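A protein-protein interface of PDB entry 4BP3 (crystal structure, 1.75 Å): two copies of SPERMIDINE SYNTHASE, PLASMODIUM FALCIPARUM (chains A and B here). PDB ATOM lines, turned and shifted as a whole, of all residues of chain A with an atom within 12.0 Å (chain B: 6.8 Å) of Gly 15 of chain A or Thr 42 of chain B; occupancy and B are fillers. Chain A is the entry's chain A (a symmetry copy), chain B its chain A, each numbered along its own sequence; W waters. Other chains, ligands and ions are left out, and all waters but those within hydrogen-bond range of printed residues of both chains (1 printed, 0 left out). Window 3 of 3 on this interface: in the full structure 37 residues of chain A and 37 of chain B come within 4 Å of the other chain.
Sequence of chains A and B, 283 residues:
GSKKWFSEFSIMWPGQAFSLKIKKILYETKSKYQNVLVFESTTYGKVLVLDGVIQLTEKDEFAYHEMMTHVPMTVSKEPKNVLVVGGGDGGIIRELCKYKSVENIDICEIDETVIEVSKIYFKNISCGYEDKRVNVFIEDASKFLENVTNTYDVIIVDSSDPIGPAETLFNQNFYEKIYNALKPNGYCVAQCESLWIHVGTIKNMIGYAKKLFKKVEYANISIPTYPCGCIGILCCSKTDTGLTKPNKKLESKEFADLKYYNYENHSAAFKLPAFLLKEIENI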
ATOM      1  N   SER A   7      22.861 -18.004 -23.046  1.00  0.00           N
ATOM      2  CA  SER A   7      21.535 -18.441 -22.661  1.00  0.00           C
ATOM      3  C   SER A   7      21.174 -19.780 -23.223  1.00  0.00           C
ATOM      4  O   SER A   7      21.349 -20.032 -24.402  1.00  0.00           O
ATOM      5  CB  SER A   7      20.470 -17.409 -23.090  1.00  0.00           C
ATOM      6  OG  SER A   7      20.742 -16.274 -22.331  1.00  0.00           O
ATOM      7  N   GLU A   8      20.616 -20.643 -22.383  1.00  0.00           N
ATOM      8  CA  GLU A   8      20.240 -21.985 -22.799  1.00  0.00           C
ATOM      9  C   GLU A   8      18.743 -22.196 -23.152  1.00  0.00           C
ATOM     10  O   GLU A   8      17.883 -22.511 -22.324  1.00  0.00           O
ATOM     11  CB  GLU A   8      20.702 -22.918 -21.679  1.00  0.00           C
ATOM     12  CG  GLU A   8      20.546 -24.351 -22.030  1.00  0.00           C
ATOM     13  CD  GLU A   8      20.756 -25.204 -20.815  1.00  0.00           C
ATOM     14  OE1 GLU A   8      20.060 -24.933 -19.779  1.00  0.00           O
ATOM     15  OE2 GLU A   8      21.596 -26.153 -20.889  1.00  0.00           O
ATOM     16  N   PHE A   9      18.404 -22.012 -24.399  1.00  0.00           N
ATOM     17  CA  PHE A   9      17.014 -22.070 -24.840  1.00  0.00           C
ATOM     18  C   PHE A   9      16.898 -23.385 -25.478  1.00  0.00           C
ATOM     19  O   PHE A   9      17.819 -23.772 -26.192  1.00  0.00           O
ATOM     20  CB  PHE A   9      16.696 -21.011 -25.945  1.00  0.00           C
ATOM     21  CG  PHE A   9      16.732 -19.593 -25.452  1.00  0.00           C
ATOM     22  CD1 PHE A   9      15.699 -19.079 -24.671  1.00  0.00           C
ATOM     23  CD2 PHE A   9      17.804 -18.778 -25.763  1.00  0.00           C
ATOM     24  CE1 PHE A   9      15.734 -17.763 -24.214  1.00  0.00           C
ATOM     25  CE2 PHE A   9      17.851 -17.475 -25.299  1.00  0.00           C
ATOM     26  CZ  PHE A   9      16.832 -16.969 -24.513  1.00  0.00           C
ATOM     27  N   SER A  10      15.750 -24.045 -25.331  1.00  0.00           N
ATOM     28  CA  SER A  10      15.538 -25.317 -26.025  1.00  0.00           C
ATOM     29  C   SER A  10      14.035 -25.700 -26.078  1.00  0.00           C
ATOM     30  O   SER A  10      13.275 -25.466 -25.128  1.00  0.00           O
ATOM     31  CB  SER A  10      16.364 -26.411 -25.307  1.00  0.00           C
ATOM     32  OG  SER A  10      16.083 -27.704 -25.789  1.00  0.00           O
ATOM     33  N   ILE A  11      13.619 -26.322 -27.154  1.00  0.00           N
ATOM     34  CA  ILE A  11      12.259 -26.889 -27.186  1.00  0.00           C
ATOM     35  C   ILE A  11      12.038 -27.989 -26.136  1.00  0.00           C
ATOM     36  O   ILE A  11      10.885 -28.367 -25.866  1.00  0.00           O
ATOM     37  CB  ILE A  11      11.874 -27.437 -28.547  1.00  0.00           C
ATOM     38  CG1 ILE A  11      12.853 -28.545 -28.948  1.00  0.00           C
ATOM     39  CG2 ILE A  11      11.809 -26.281 -29.558  1.00  0.00           C
ATOM     40  CD1 ILE A  11      12.310 -29.393 -30.061  1.00  0.00           C
ATOM     41  N   MET A  12      13.137 -28.552 -25.622  1.00  0.00           N
ATOM     42  CA  MET A  12      13.077 -29.565 -24.582  1.00  0.00           C
ATOM     43  C   MET A  12      12.663 -28.967 -23.233  1.00  0.00           C
ATOM     44  O   MET A  12      12.292 -29.660 -22.299  1.00  0.00           O
ATOM     45  CB  MET A  12      14.406 -30.312 -24.475  1.00  0.00           C
ATOM     46  CG  MET A  12      14.775 -31.032 -25.762  1.00  0.00           C
ATOM     47  SD  MET A  12      16.284 -31.964 -25.466  1.00  0.00           S
ATOM     48  CE  MET A  12      17.592 -30.721 -25.409  1.00  0.00           C
ATOM     49  N   TRP A  13      12.689 -27.652 -23.156  1.00  0.00           N
ATOM     50  CA  TRP A  13      12.215 -26.962 -21.948  1.00  0.00           C
ATOM     51  C   TRP A  13      11.627 -25.629 -22.428  1.00  0.00           C
ATOM     52  O   TRP A  13      12.167 -24.551 -22.172  1.00  0.00           O
ATOM     53  CB  TRP A  13      13.285 -26.795 -20.890  1.00  0.00           C
ATOM     54  CG  TRP A  13      14.745 -26.501 -21.325  1.00  0.00           C
ATOM     55  CD1 TRP A  13      15.275 -25.317 -21.571  1.00  0.00           C
ATOM     56  CD2 TRP A  13      15.791 -27.478 -21.610  1.00  0.00           C
ATOM     57  NE1 TRP A  13      16.617 -25.437 -21.931  1.00  0.00           N
ATOM     58  CE2 TRP A  13      16.952 -26.762 -21.926  1.00  0.00           C
ATOM     59  CE3 TRP A  13      15.846 -28.851 -21.537  1.00  0.00           C
ATOM     60  CZ2 TRP A  13      18.141 -27.373 -22.279  1.00  0.00           C
ATOM     61  CZ3 TRP A  13      17.043 -29.479 -21.856  1.00  0.00           C
ATOM     62  CH2 TRP A  13      18.169 -28.737 -22.229  1.00  0.00           C
ATOM     63  N   PRO A  14      10.501 -25.728 -23.104  1.00  0.00           N
ATOM     64  CA  PRO A  14       9.969 -24.484 -23.693  1.00  0.00           C
ATOM     65  C   PRO A  14       9.525 -23.527 -22.595  1.00  0.00           C
ATOM     66  O   PRO A  14       9.039 -23.959 -21.526  1.00  0.00           O
ATOM     67  CB  PRO A  14       8.747 -24.988 -24.491  1.00  0.00           C
ATOM     68  CG  PRO A  14       8.289 -26.236 -23.735  1.00  0.00           C
ATOM     69  CD  PRO A  14       9.569 -26.884 -23.262  1.00  0.00           C
ATOM     70  N   GLY A  15       9.687 -22.235 -22.839  1.00  0.00           N
ATOM     71  CA  GLY A  15       9.141 -21.247 -21.927  1.00  0.00           C
ATOM     72  C   GLY A  15      10.040 -20.916 -20.815  1.00  0.00           C
ATOM     73  O   GLY A  15       9.712 -20.074 -20.053  1.00  0.00           O
ATOM     74  N   GLN A  16      11.229 -21.533 -20.756  1.00  0.00           N
ATOM     75  CA  GLN A  16      12.196 -21.291 -19.717  1.00  0.00           C
ATOM     76  C   GLN A  16      13.604 -21.254 -20.234  1.00  0.00           C
ATOM     77  O   GLN A  16      13.876 -21.830 -21.256  1.00  0.00           O
ATOM     78  CB  GLN A  16      12.092 -22.357 -18.626  1.00  0.00           C
ATOM     79  CG  GLN A  16      12.761 -23.662 -18.948  1.00  0.00           C
ATOM     80  CD  GLN A  16      12.604 -24.694 -17.876  1.00  0.00           C
ATOM     81  OE1 GLN A  16      13.605 -25.029 -17.155  1.00  0.00           O
ATOM     82  NE2 GLN A  16      11.414 -25.267 -17.781  1.00  0.00           N
ATOM     83  N   ALA A  17      14.491 -20.575 -19.533  1.00  0.00           N
ATOM     84  CA  ALA A  17      15.905 -20.519 -19.918  1.00  0.00           C
ATOM     85  C   ALA A  17      16.802 -20.170 -18.785  1.00  0.00           C
ATOM     86  O   ALA A  17      16.493 -19.313 -17.892  1.00  0.00           O
ATOM     87  CB  ALA A  17      16.134 -19.596 -21.145  1.00  0.00           C
ATOM     88  N   PHE A  18      17.973 -20.818 -18.746  1.00  0.00           N
ATOM     89  CA  PHE A  18      19.031 -20.437 -17.773  1.00  0.00           C
ATOM     90  C   PHE A  18      20.180 -19.752 -18.515  1.00  0.00           C
ATOM     91  O   PHE A  18      20.541 -20.179 -19.626  1.00  0.00           O
ATOM     92  CB  PHE A  18      19.567 -21.717 -17.022  1.00  0.00           C
ATOM     93  CG  PHE A  18      20.681 -21.451 -16.029  1.00  0.00           C
ATOM     94  CD1 PHE A  18      20.390 -20.853 -14.860  1.00  0.00           C
ATOM     95  CD2 PHE A  18      22.018 -21.889 -16.238  1.00  0.00           C
ATOM     96  CE1 PHE A  18      21.384 -20.585 -13.936  1.00  0.00           C
ATOM     97  CE2 PHE A  18      23.024 -21.661 -15.293  1.00  0.00           C
ATOM     98  CZ  PHE A  18      22.697 -21.005 -14.126  1.00  0.00           C
ATOM     99  N   SER A  19      20.802 -18.745 -17.893  1.00  0.00           N
ATOM    100  CA  SER A  19      21.945 -17.986 -18.512  1.00  0.00           C
ATOM    101  C   SER A  19      23.136 -17.829 -17.586  1.00  0.00           C
ATOM    102  O   SER A  19      22.972 -17.709 -16.396  1.00  0.00           O
ATOM    103  CB  SER A  19      21.473 -16.565 -18.915  1.00  0.00           C
ATOM    104  OG  SER A  19      20.381 -16.672 -19.804  1.00  0.00           O
ATOM    105  N   TRP A 196      10.760 -32.113 -13.234  1.00  0.00           N
ATOM    106  CA  TRP A 196       9.809 -30.971 -13.290  1.00  0.00           C
ATOM    107  C   TRP A 196       9.139 -30.781 -14.637  1.00  0.00           C
ATOM    108  O   TRP A 196       8.036 -30.196 -14.742  1.00  0.00           O
ATOM    109  CB  TRP A 196      10.538 -29.752 -12.835  1.00  0.00           C
ATOM    110  CG  TRP A 196      10.611 -29.724 -11.476  1.00  0.00           C
ATOM    111  CD1 TRP A 196      11.710 -29.944 -10.669  1.00  0.00           C
ATOM    112  CD2 TRP A 196       9.522 -29.438 -10.605  1.00  0.00           C
ATOM    113  NE1 TRP A 196      11.336 -29.860  -9.352  1.00  0.00           N
ATOM    114  CE2 TRP A 196      10.009 -29.524  -9.289  1.00  0.00           C
ATOM    115  CE3 TRP A 196       8.195 -29.100 -10.826  1.00  0.00           C
ATOM    116  CZ2 TRP A 196       9.230 -29.273  -8.192  1.00  0.00           C
ATOM    117  CZ3 TRP A 196       7.401 -28.825  -9.679  1.00  0.00           C
ATOM    118  CH2 TRP A 196       7.910 -28.926  -8.429  1.00  0.00           C
ATOM    119  N   ILE A 197       9.783 -31.251 -15.708  1.00  0.00           N
ATOM    120  CA  ILE A 197       9.296 -30.962 -17.027  1.00  0.00           C
ATOM    121  C   ILE A 197       9.345 -32.099 -17.977  1.00  0.00           C
ATOM    122  O   ILE A 197       8.738 -32.019 -19.024  1.00  0.00           O
ATOM    123  CB  ILE A 197      10.070 -29.810 -17.693  1.00  0.00           C
ATOM    124  CG1 ILE A 197      11.624 -30.023 -17.572  1.00  0.00           C
ATOM    125  CG2 ILE A 197       9.555 -28.486 -17.142  1.00  0.00           C
ATOM    126  CD1 ILE A 197      12.472 -28.983 -18.265  1.00  0.00           C
ATOM    127  N   HIS A 198       9.983 -33.204 -17.595  1.00  0.00           N
ATOM    128  CA  HIS A 198      10.211 -34.280 -18.545  1.00  0.00           C
ATOM    129  C   HIS A 198       9.543 -35.567 -18.078  1.00  0.00           C
ATOM    130  O   HIS A 198      10.063 -36.675 -18.293  1.00  0.00           O
ATOM    131  CB  HIS A 198      11.740 -34.500 -18.685  1.00  0.00           C
ATOM    132  CG  HIS A 198      12.447 -33.328 -19.268  1.00  0.00           C
ATOM    133  ND1 HIS A 198      13.673 -32.879 -18.820  1.00  0.00           N
ATOM    134  CD2 HIS A 198      12.090 -32.507 -20.277  1.00  0.00           C
ATOM    135  CE1 HIS A 198      14.025 -31.803 -19.508  1.00  0.00           C
ATOM    136  NE2 HIS A 198      13.091 -31.580 -20.424  1.00  0.00           N
ATOM    137  N   PRO A 227      18.796 -27.931 -16.516  1.00  0.00           N
ATOM    138  CA  PRO A 227      17.464 -27.240 -16.521  1.00  0.00           C
ATOM    139  C   PRO A 227      16.569 -27.700 -15.379  1.00  0.00           C
ATOM    140  O   PRO A 227      16.524 -28.886 -15.060  1.00  0.00           O
ATOM    141  CB  PRO A 227      16.835 -27.737 -17.794  1.00  0.00           C
ATOM    142  CG  PRO A 227      18.030 -27.836 -18.711  1.00  0.00           C
ATOM    143  CD  PRO A 227      19.143 -28.390 -17.861  1.00  0.00           C
ATOM    144  N   CYS A 228      15.946 -26.732 -14.732  1.00  0.00           N
ATOM    145  CA  CYS A 228      15.137 -26.977 -13.542  1.00  0.00           C
ATOM    146  C   CYS A 228      15.971 -27.255 -12.306  1.00  0.00           C
ATOM    147  O   CYS A 228      15.412 -27.432 -11.223  1.00  0.00           O
ATOM    148  CB  CYS A 228      14.071 -28.022 -13.791  1.00  0.00           C
ATOM    149  SG  CYS A 228      12.755 -27.522 -14.946  1.00  0.00           S
ATOM    150  N   LYS B   3       6.512 -12.513 -28.491  1.00  0.00           N
ATOM    151  CA  LYS B   3       6.446 -12.765 -27.005  1.00  0.00           C
ATOM    152  C   LYS B   3       7.777 -12.400 -26.270  1.00  0.00           C
ATOM    153  O   LYS B   3       8.874 -12.685 -26.701  1.00  0.00           O
ATOM    154  CB  LYS B   3       5.957 -14.192 -26.649  1.00  0.00           C
ATOM    155  CG  LYS B   3       4.436 -14.385 -26.755  1.00  0.00           C
ATOM    156  CD  LYS B   3       3.988 -15.754 -26.228  1.00  0.00           C
ATOM    157  CE  LYS B   3       2.481 -16.013 -26.334  1.00  0.00           C
ATOM    158  NZ  LYS B   3       1.587 -14.854 -25.966  1.00  0.00           N
ATOM    159  N   LYS B   4       7.633 -11.732 -25.153  1.00  0.00           N
ATOM    160  CA  LYS B   4       8.739 -11.188 -24.371  1.00  0.00           C
ATOM    161  C   LYS B   4       9.080 -12.297 -23.325  1.00  0.00           C
ATOM    162  O   LYS B   4       8.262 -13.167 -23.066  1.00  0.00           O
ATOM    163  CB  LYS B   4       8.160  -9.939 -23.672  1.00  0.00           C
ATOM    164  CG  LYS B   4       9.100  -8.823 -23.302  1.00  0.00           C
ATOM    165  CD  LYS B   4       9.078  -7.649 -24.284  1.00  0.00           C
ATOM    166  CE  LYS B   4      10.316  -6.781 -24.052  1.00  0.00           C
ATOM    167  NZ  LYS B   4      11.548  -7.645 -23.876  1.00  0.00           N
ATOM    168  N   TRP B   5      10.256 -12.192 -22.710  1.00  0.00           N
ATOM    169  CA  TRP B   5      10.654 -12.994 -21.570  1.00  0.00           C
ATOM    170  C   TRP B   5      10.885 -12.153 -20.305  1.00  0.00           C
ATOM    171  O   TRP B   5      11.399 -11.059 -20.381  1.00  0.00           O
ATOM    172  CB  TRP B   5      12.009 -13.608 -21.889  1.00  0.00           C
ATOM    173  CG  TRP B   5      11.869 -14.664 -22.950  1.00  0.00           C
ATOM    174  CD1 TRP B   5      11.638 -14.462 -24.302  1.00  0.00           C
ATOM    175  CD2 TRP B   5      12.063 -16.074 -22.775  1.00  0.00           C
ATOM    176  NE1 TRP B   5      11.576 -15.699 -24.952  1.00  0.00           N
ATOM    177  CE2 TRP B   5      11.850 -16.697 -24.041  1.00  0.00           C
ATOM    178  CE3 TRP B   5      12.307 -16.877 -21.670  1.00  0.00           C
ATOM    179  CZ2 TRP B   5      11.928 -18.097 -24.215  1.00  0.00           C
ATOM    180  CZ3 TRP B   5      12.398 -18.250 -21.832  1.00  0.00           C
ATOM    181  CH2 TRP B   5      12.203 -18.858 -23.102  1.00  0.00           C
ATOM    182  N   PHE B  18      17.780 -16.845 -14.410  1.00  0.00           N
ATOM    183  CA  PHE B  18      16.695 -17.715 -14.936  1.00  0.00           C
ATOM    184  C   PHE B  18      15.631 -16.849 -15.612  1.00  0.00           C
ATOM    185  O   PHE B  18      15.307 -15.760 -15.106  1.00  0.00           O
ATOM    186  CB  PHE B  18      16.043 -18.542 -13.761  1.00  0.00           C
ATOM    187  CG  PHE B  18      14.894 -19.440 -14.178  1.00  0.00           C
ATOM    188  CD1 PHE B  18      15.156 -20.567 -14.862  1.00  0.00           C
ATOM    189  CD2 PHE B  18      13.547 -19.191 -13.796  1.00  0.00           C
ATOM    190  CE1 PHE B  18      14.131 -21.403 -15.268  1.00  0.00           C
ATOM    191  CE2 PHE B  18      12.506 -20.050 -14.164  1.00  0.00           C
ATOM    192  CZ  PHE B  18      12.808 -21.172 -14.905  1.00  0.00           C
ATOM    193  N   SER B  19      15.037 -17.341 -16.704  1.00  0.00           N
ATOM    194  CA  SER B  19      13.978 -16.590 -17.465  1.00  0.00           C
ATOM    195  C   SER B  19      12.750 -17.425 -17.771  1.00  0.00           C
ATOM    196  O   SER B  19      12.855 -18.608 -17.989  1.00  0.00           O
ATOM    197  CB  SER B  19      14.555 -16.093 -18.815  1.00  0.00           C
ATOM    198  OG  SER B  19      15.686 -15.284 -18.568  1.00  0.00           O
ATOM    199  N   LEU B  20      11.582 -16.802 -17.813  1.00  0.00           N
ATOM    200  CA  LEU B  20      10.321 -17.439 -18.224  1.00  0.00           C
ATOM    201  C   LEU B  20       9.644 -16.648 -19.328  1.00  0.00           C
ATOM    202  O   LEU B  20       9.554 -15.401 -19.270  1.00  0.00           O
ATOM    203  CB  LEU B  20       9.293 -17.472 -17.123  1.00  0.00           C
ATOM    204  CG  LEU B  20       9.662 -18.357 -15.949  1.00  0.00           C
ATOM    205  CD1 LEU B  20       8.659 -18.141 -14.841  1.00  0.00           C
ATOM    206  CD2 LEU B  20       9.563 -19.799 -16.369  1.00  0.00           C
ATOM    207  N   LYS B  21       9.072 -17.353 -20.292  1.00  0.00           N
ATOM    208  CA  LYS B  21       8.411 -16.663 -21.354  1.00  0.00           C
ATOM    209  C   LYS B  21       7.026 -16.187 -20.936  1.00  0.00           C
ATOM    210  O   LYS B  21       6.275 -16.880 -20.252  1.00  0.00           O
ATOM    211  CB  LYS B  21       8.247 -17.570 -22.525  1.00  0.00           C
ATOM    212  CG  LYS B  21       7.812 -16.859 -23.769  1.00  0.00           C
ATOM    213  CD  LYS B  21       7.939 -17.833 -24.933  1.00  0.00           C
ATOM    214  CE  LYS B  21       7.611 -17.093 -26.214  1.00  0.00           C
ATOM    215  NZ  LYS B  21       7.717 -18.004 -27.390  1.00  0.00           N
ATOM    216  N   ILE B  22       6.716 -14.980 -21.385  1.00  0.00           N
ATOM    217  CA  ILE B  22       5.466 -14.290 -20.951  1.00  0.00           C
ATOM    218  C   ILE B  22       4.359 -14.492 -21.982  1.00  0.00           C
ATOM    219  O   ILE B  22       4.498 -14.006 -23.099  1.00  0.00           O
ATOM    220  CB  ILE B  22       5.683 -12.796 -20.814  1.00  0.00           C
ATOM    221  CG1 ILE B  22       6.797 -12.471 -19.772  1.00  0.00           C
ATOM    222  CG2 ILE B  22       4.324 -12.092 -20.448  1.00  0.00           C
ATOM    223  CD1 ILE B  22       7.546 -11.113 -19.831  1.00  0.00           C
ATOM    224  N   LYS B  23       3.252 -15.082 -21.551  1.00  0.00           N
ATOM    225  CA  LYS B  23       2.004 -15.144 -22.317  1.00  0.00           C
ATOM    226  C   LYS B  23       1.282 -13.791 -22.228  1.00  0.00           C
ATOM    227  O   LYS B  23       0.998 -13.198 -23.236  1.00  0.00           O
ATOM    228  CB  LYS B  23       1.078 -16.185 -21.832  1.00  0.00           C
ATOM    229  CG  LYS B  23      -0.062 -16.386 -22.840  1.00  0.00           C
ATOM    230  CD  LYS B  23      -0.996 -17.437 -22.343  1.00  0.00           C
ATOM    231  CE  LYS B  23      -1.734 -18.061 -23.496  1.00  0.00           C
ATOM    232  NZ  LYS B  23      -2.987 -18.600 -22.908  1.00  0.00           N
ATOM    233  N   LYS B  24       1.006 -13.316 -21.026  1.00  0.00           N
ATOM    234  CA  LYS B  24       0.470 -11.940 -20.902  1.00  0.00           C
ATOM    235  C   LYS B  24       0.747 -11.380 -19.538  1.00  0.00           C
ATOM    236  O   LYS B  24       0.794 -12.129 -18.582  1.00  0.00           O
ATOM    237  CB  LYS B  24      -0.986 -11.875 -21.298  1.00  0.00           C
ATOM    238  CG  LYS B  24      -1.951 -12.806 -20.608  1.00  0.00           C
ATOM    239  CD  LYS B  24      -3.383 -12.305 -20.881  1.00  0.00           C
ATOM    240  CE  LYS B  24      -3.494 -10.800 -20.596  1.00  0.00           C
ATOM    241  NZ  LYS B  24      -4.890 -10.278 -20.627  1.00  0.00           N
ATOM    242  N   PHE B  39       2.255 -12.161 -14.083  1.00  0.00           N
ATOM    243  CA  PHE B  39       2.140 -12.455 -15.502  1.00  0.00           C
ATOM    244  C   PHE B  39       1.749 -13.892 -15.649  1.00  0.00           C
ATOM    245  O   PHE B  39       2.031 -14.694 -14.769  1.00  0.00           O
ATOM    246  CB  PHE B  39       3.405 -12.049 -16.268  1.00  0.00           C
ATOM    247  CG  PHE B  39       4.678 -12.859 -15.960  1.00  0.00           C
ATOM    248  CD1 PHE B  39       5.019 -13.921 -16.701  1.00  0.00           C
ATOM    249  CD2 PHE B  39       5.585 -12.404 -15.030  1.00  0.00           C
ATOM    250  CE1 PHE B  39       6.223 -14.649 -16.433  1.00  0.00           C
ATOM    251  CE2 PHE B  39       6.778 -13.046 -14.769  1.00  0.00           C
ATOM    252  CZ  PHE B  39       7.097 -14.198 -15.456  1.00  0.00           C
ATOM    253  N   GLU B  40       1.007 -14.196 -16.700  1.00  0.00           N
ATOM    254  CA  GLU B  40       0.792 -15.551 -17.101  1.00  0.00           C
ATOM    255  C   GLU B  40       2.024 -15.931 -17.957  1.00  0.00           C
ATOM    256  O   GLU B  40       2.296 -15.277 -18.926  1.00  0.00           O
ATOM    257  CB  GLU B  40      -0.489 -15.682 -17.907  1.00  0.00           C
ATOM    258  CG  GLU B  40      -1.394 -16.720 -17.329  1.00  0.00           C
ATOM    259  CD  GLU B  40      -1.618 -17.899 -18.184  1.00  0.00           C
ATOM    260  OE1 GLU B  40      -2.176 -17.692 -19.266  1.00  0.00           O
ATOM    261  OE2 GLU B  40      -1.326 -19.033 -17.704  1.00  0.00           O
ATOM    262  N   SER B  41       2.773 -16.954 -17.550  1.00  0.00           N
ATOM    263  CA  SER B  41       3.892 -17.447 -18.318  1.00  0.00           C
ATOM    264  C   SER B  41       3.289 -18.419 -19.312  1.00  0.00           C
ATOM    265  O   SER B  41       2.127 -18.861 -19.174  1.00  0.00           O
ATOM    266  CB  SER B  41       4.917 -18.160 -17.427  1.00  0.00           C
ATOM    267  OG  SER B  41       4.385 -19.364 -16.885  1.00  0.00           O
ATOM    268  N   THR B  42       4.089 -18.817 -20.276  1.00  0.00           N
ATOM    269  CA  THR B  42       3.557 -19.763 -21.289  1.00  0.00           C
ATOM    270  C   THR B  42       3.483 -21.184 -20.741  1.00  0.00           C
ATOM    271  O   THR B  42       2.636 -21.967 -21.113  1.00  0.00           O
ATOM    272  CB  THR B  42       4.437 -19.675 -22.552  1.00  0.00           C
ATOM    273  OG1 THR B  42       5.793 -19.926 -22.203  1.00  0.00           O
ATOM    274  CG2 THR B  42       4.374 -18.272 -23.134  1.00  0.00           C
ATOM    275  N   THR B  43       4.388 -21.531 -19.849  1.00  0.00           N
ATOM    276  CA  THR B  43       4.470 -22.918 -19.375  1.00  0.00           C
ATOM    277  C   THR B  43       4.430 -23.148 -17.909  1.00  0.00           C
ATOM    278  O   THR B  43       4.281 -24.285 -17.499  1.00  0.00           O
ATOM    279  CB  THR B  43       5.674 -23.657 -20.040  1.00  0.00           C
ATOM    280  OG1 THR B  43       6.920 -23.067 -19.641  1.00  0.00           O
ATOM    281  CG2 THR B  43       5.591 -23.488 -21.478  1.00  0.00           C
ATOM    282  N   TYR B  44       4.588 -22.110 -17.089  1.00  0.00           N
ATOM    283  CA  TYR B  44       4.561 -22.268 -15.649  1.00  0.00           C
ATOM    284  C   TYR B  44       3.330 -21.651 -14.972  1.00  0.00           C
ATOM    285  O   TYR B  44       3.286 -21.536 -13.718  1.00  0.00           O
ATOM    286  CB  TYR B  44       5.848 -21.717 -15.006  1.00  0.00           C
ATOM    287  CG  TYR B  44       7.062 -22.666 -15.122  1.00  0.00           C
ATOM    288  CD1 TYR B  44       7.603 -23.003 -16.350  1.00  0.00           C
ATOM    289  CD2 TYR B  44       7.693 -23.166 -13.989  1.00  0.00           C
ATOM    290  CE1 TYR B  44       8.727 -23.888 -16.449  1.00  0.00           C
ATOM    291  CE2 TYR B  44       8.802 -24.029 -14.054  1.00  0.00           C
ATOM    292  CZ  TYR B  44       9.312 -24.384 -15.287  1.00  0.00           C
ATOM    293  OH  TYR B  44      10.411 -25.235 -15.285  1.00  0.00           O
ATOM    294  N   GLY B  45       2.343 -21.351 -15.800  1.00  0.00           N
ATOM    295  CA  GLY B  45       1.112 -20.704 -15.369  1.00  0.00           C
ATOM    296  C   GLY B  45       1.410 -19.321 -14.890  1.00  0.00           C
ATOM    297  O   GLY B  45       2.332 -18.687 -15.368  1.00  0.00           O
HETATM  298  O   HOH W   1       6.933 -20.170 -19.093  1.00  0.00           O
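Gly 15 of chain A touches Trp 5 of chain B (C to CZ3, 3.7 Å).
Thr 42 of chain B touches Gly 15 of chain A (OG1 to CA, 3.6 Å).
Gly 15 of chain A touches Thr 43 of chain B (CA to OG1, 3.7 Å).
Gln 16 of chain A touches Trp 5 of chain B (C to CZ3, 3.6 Å).
CB of Gln 16 of chain A touches CZ of Phe 18 of chain B (3.97 Å).
O of Ser 19 of chain B touches CA of Gln 16 of chain A (3.3 Å).
Ala 17 of chain A touches Trp 5 of chain B.
Phe 18 of chain B touches Ala 17 of chain A (CA to O, 3.4 Å).
Ile 197 of chain A touches Tyr 44 of chain B.
Printed residues of chain B within 4 Å of Phe 9 of chain A: Trp 5 (3.8 Å).
Trp 196 of chain A touches none of the printed residues of chain B.
Printed residues of chain A within 4 Å of Trp 5 of chain B: Phe 9, Gly 15, Gln 16 and Ala 17.
Ser 19 of chain B touches just these residues of chain A: Gln 16 (3.3 Å) and Ala 17 (2.7 Å).
Lys 21 of chain B touches just one residue of chain A: Gly 15.
No residue of chain A comes within 4 Å of Glu 40 of chain B.
No residue of chain A comes within 4 Å of Ser 41 of chain B.
Thr 42 of chain B touches one residue of chain A.
Thr 43 of chain B touches just these residues of chain A: Pro 14 and Gly 15.
Gly 45 of chain B touches none of the printed residues of chain A.
The nearest residue of chain A that does not touch Thr 42 of chain B is Pro 14 of chain A (5.2 Å).
Positions printed for both chains: 18 and 19.
Water W1 lies within hydrogen-bond range of O of Gly 15 of chain A (2.9 Å), OG1 of Thr 43 of chain B (2.9 Å), OG1 of Thr 42 of chain B (3.3 Å) and OG of Ser 41 of chain B (3.5 Å).
N of Ser 19 of chain B sits at hydrogen-bond distance from O of Ala 17 of chain A, at 2.7 Å.
The backbone carbonyl oxygen (O) of Gly 15 of chain A lies within hydrogen-bond range of the backbone NH (N) of Lys 21 of chain B (2.8 Å).
OG1 of Thr 43 of chain B is in hydrogen-bond range of O of Pro 14 of chain A, at 3.0 Å.
The side-chain hydroxyl (OH) of Tyr 44 of chain B is in hydrogen-bond range of the side-chain amide nitrogen (NE2) of Gln 16 of chain A.
The side-chain hydroxyl (OH) of Tyr 44 of chain B is in hydrogen-bond range of the side-chain sulfur (SG) of Cys 228 of chain A, at 3.3 Å.
The backbone carbonyl oxygen (O) of Lys 21 of chain B is in hydrogen-bond range of the backbone NH (N) of Thr 42 of chain B (2.9 Å).
N of Tyr 44 of chain B is in hydrogen-bond range of OG of Ser 41 of chain B (2.8 Å).
The side-chain amide oxygen (OE1) of Gln 16 of chain A lies within hydrogen-bond range of the side-chain sulfur (SG) of Cys 228 of chain A, at 3.4 Å.
Printed residues of chain A that touch a printed residue of chain B: Phe 9, Pro 14, Gly 15, Gln 16, Ala 17, Ile 197 and Cys 228.
Hydrophobic or aromatic side chains of chain A within 4 Å of the printed part of chain B: Phe 9 and Ile 197.
Of the 17 printed residues of chain B, 8 touch a printed residue of chain A.
Hydrophobic or aromatic side chains of chain B within 4 Å of the printed part of chain A: Trp 5, Phe 18, Leu 20 and Tyr 44.
Among the printed residues, 16 pairs touch across the chains.
Among the printed residues, no Asp or Glu carboxylate lies within 4 Å of a Lys or Arg side-chain nitrogen of the other chain.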
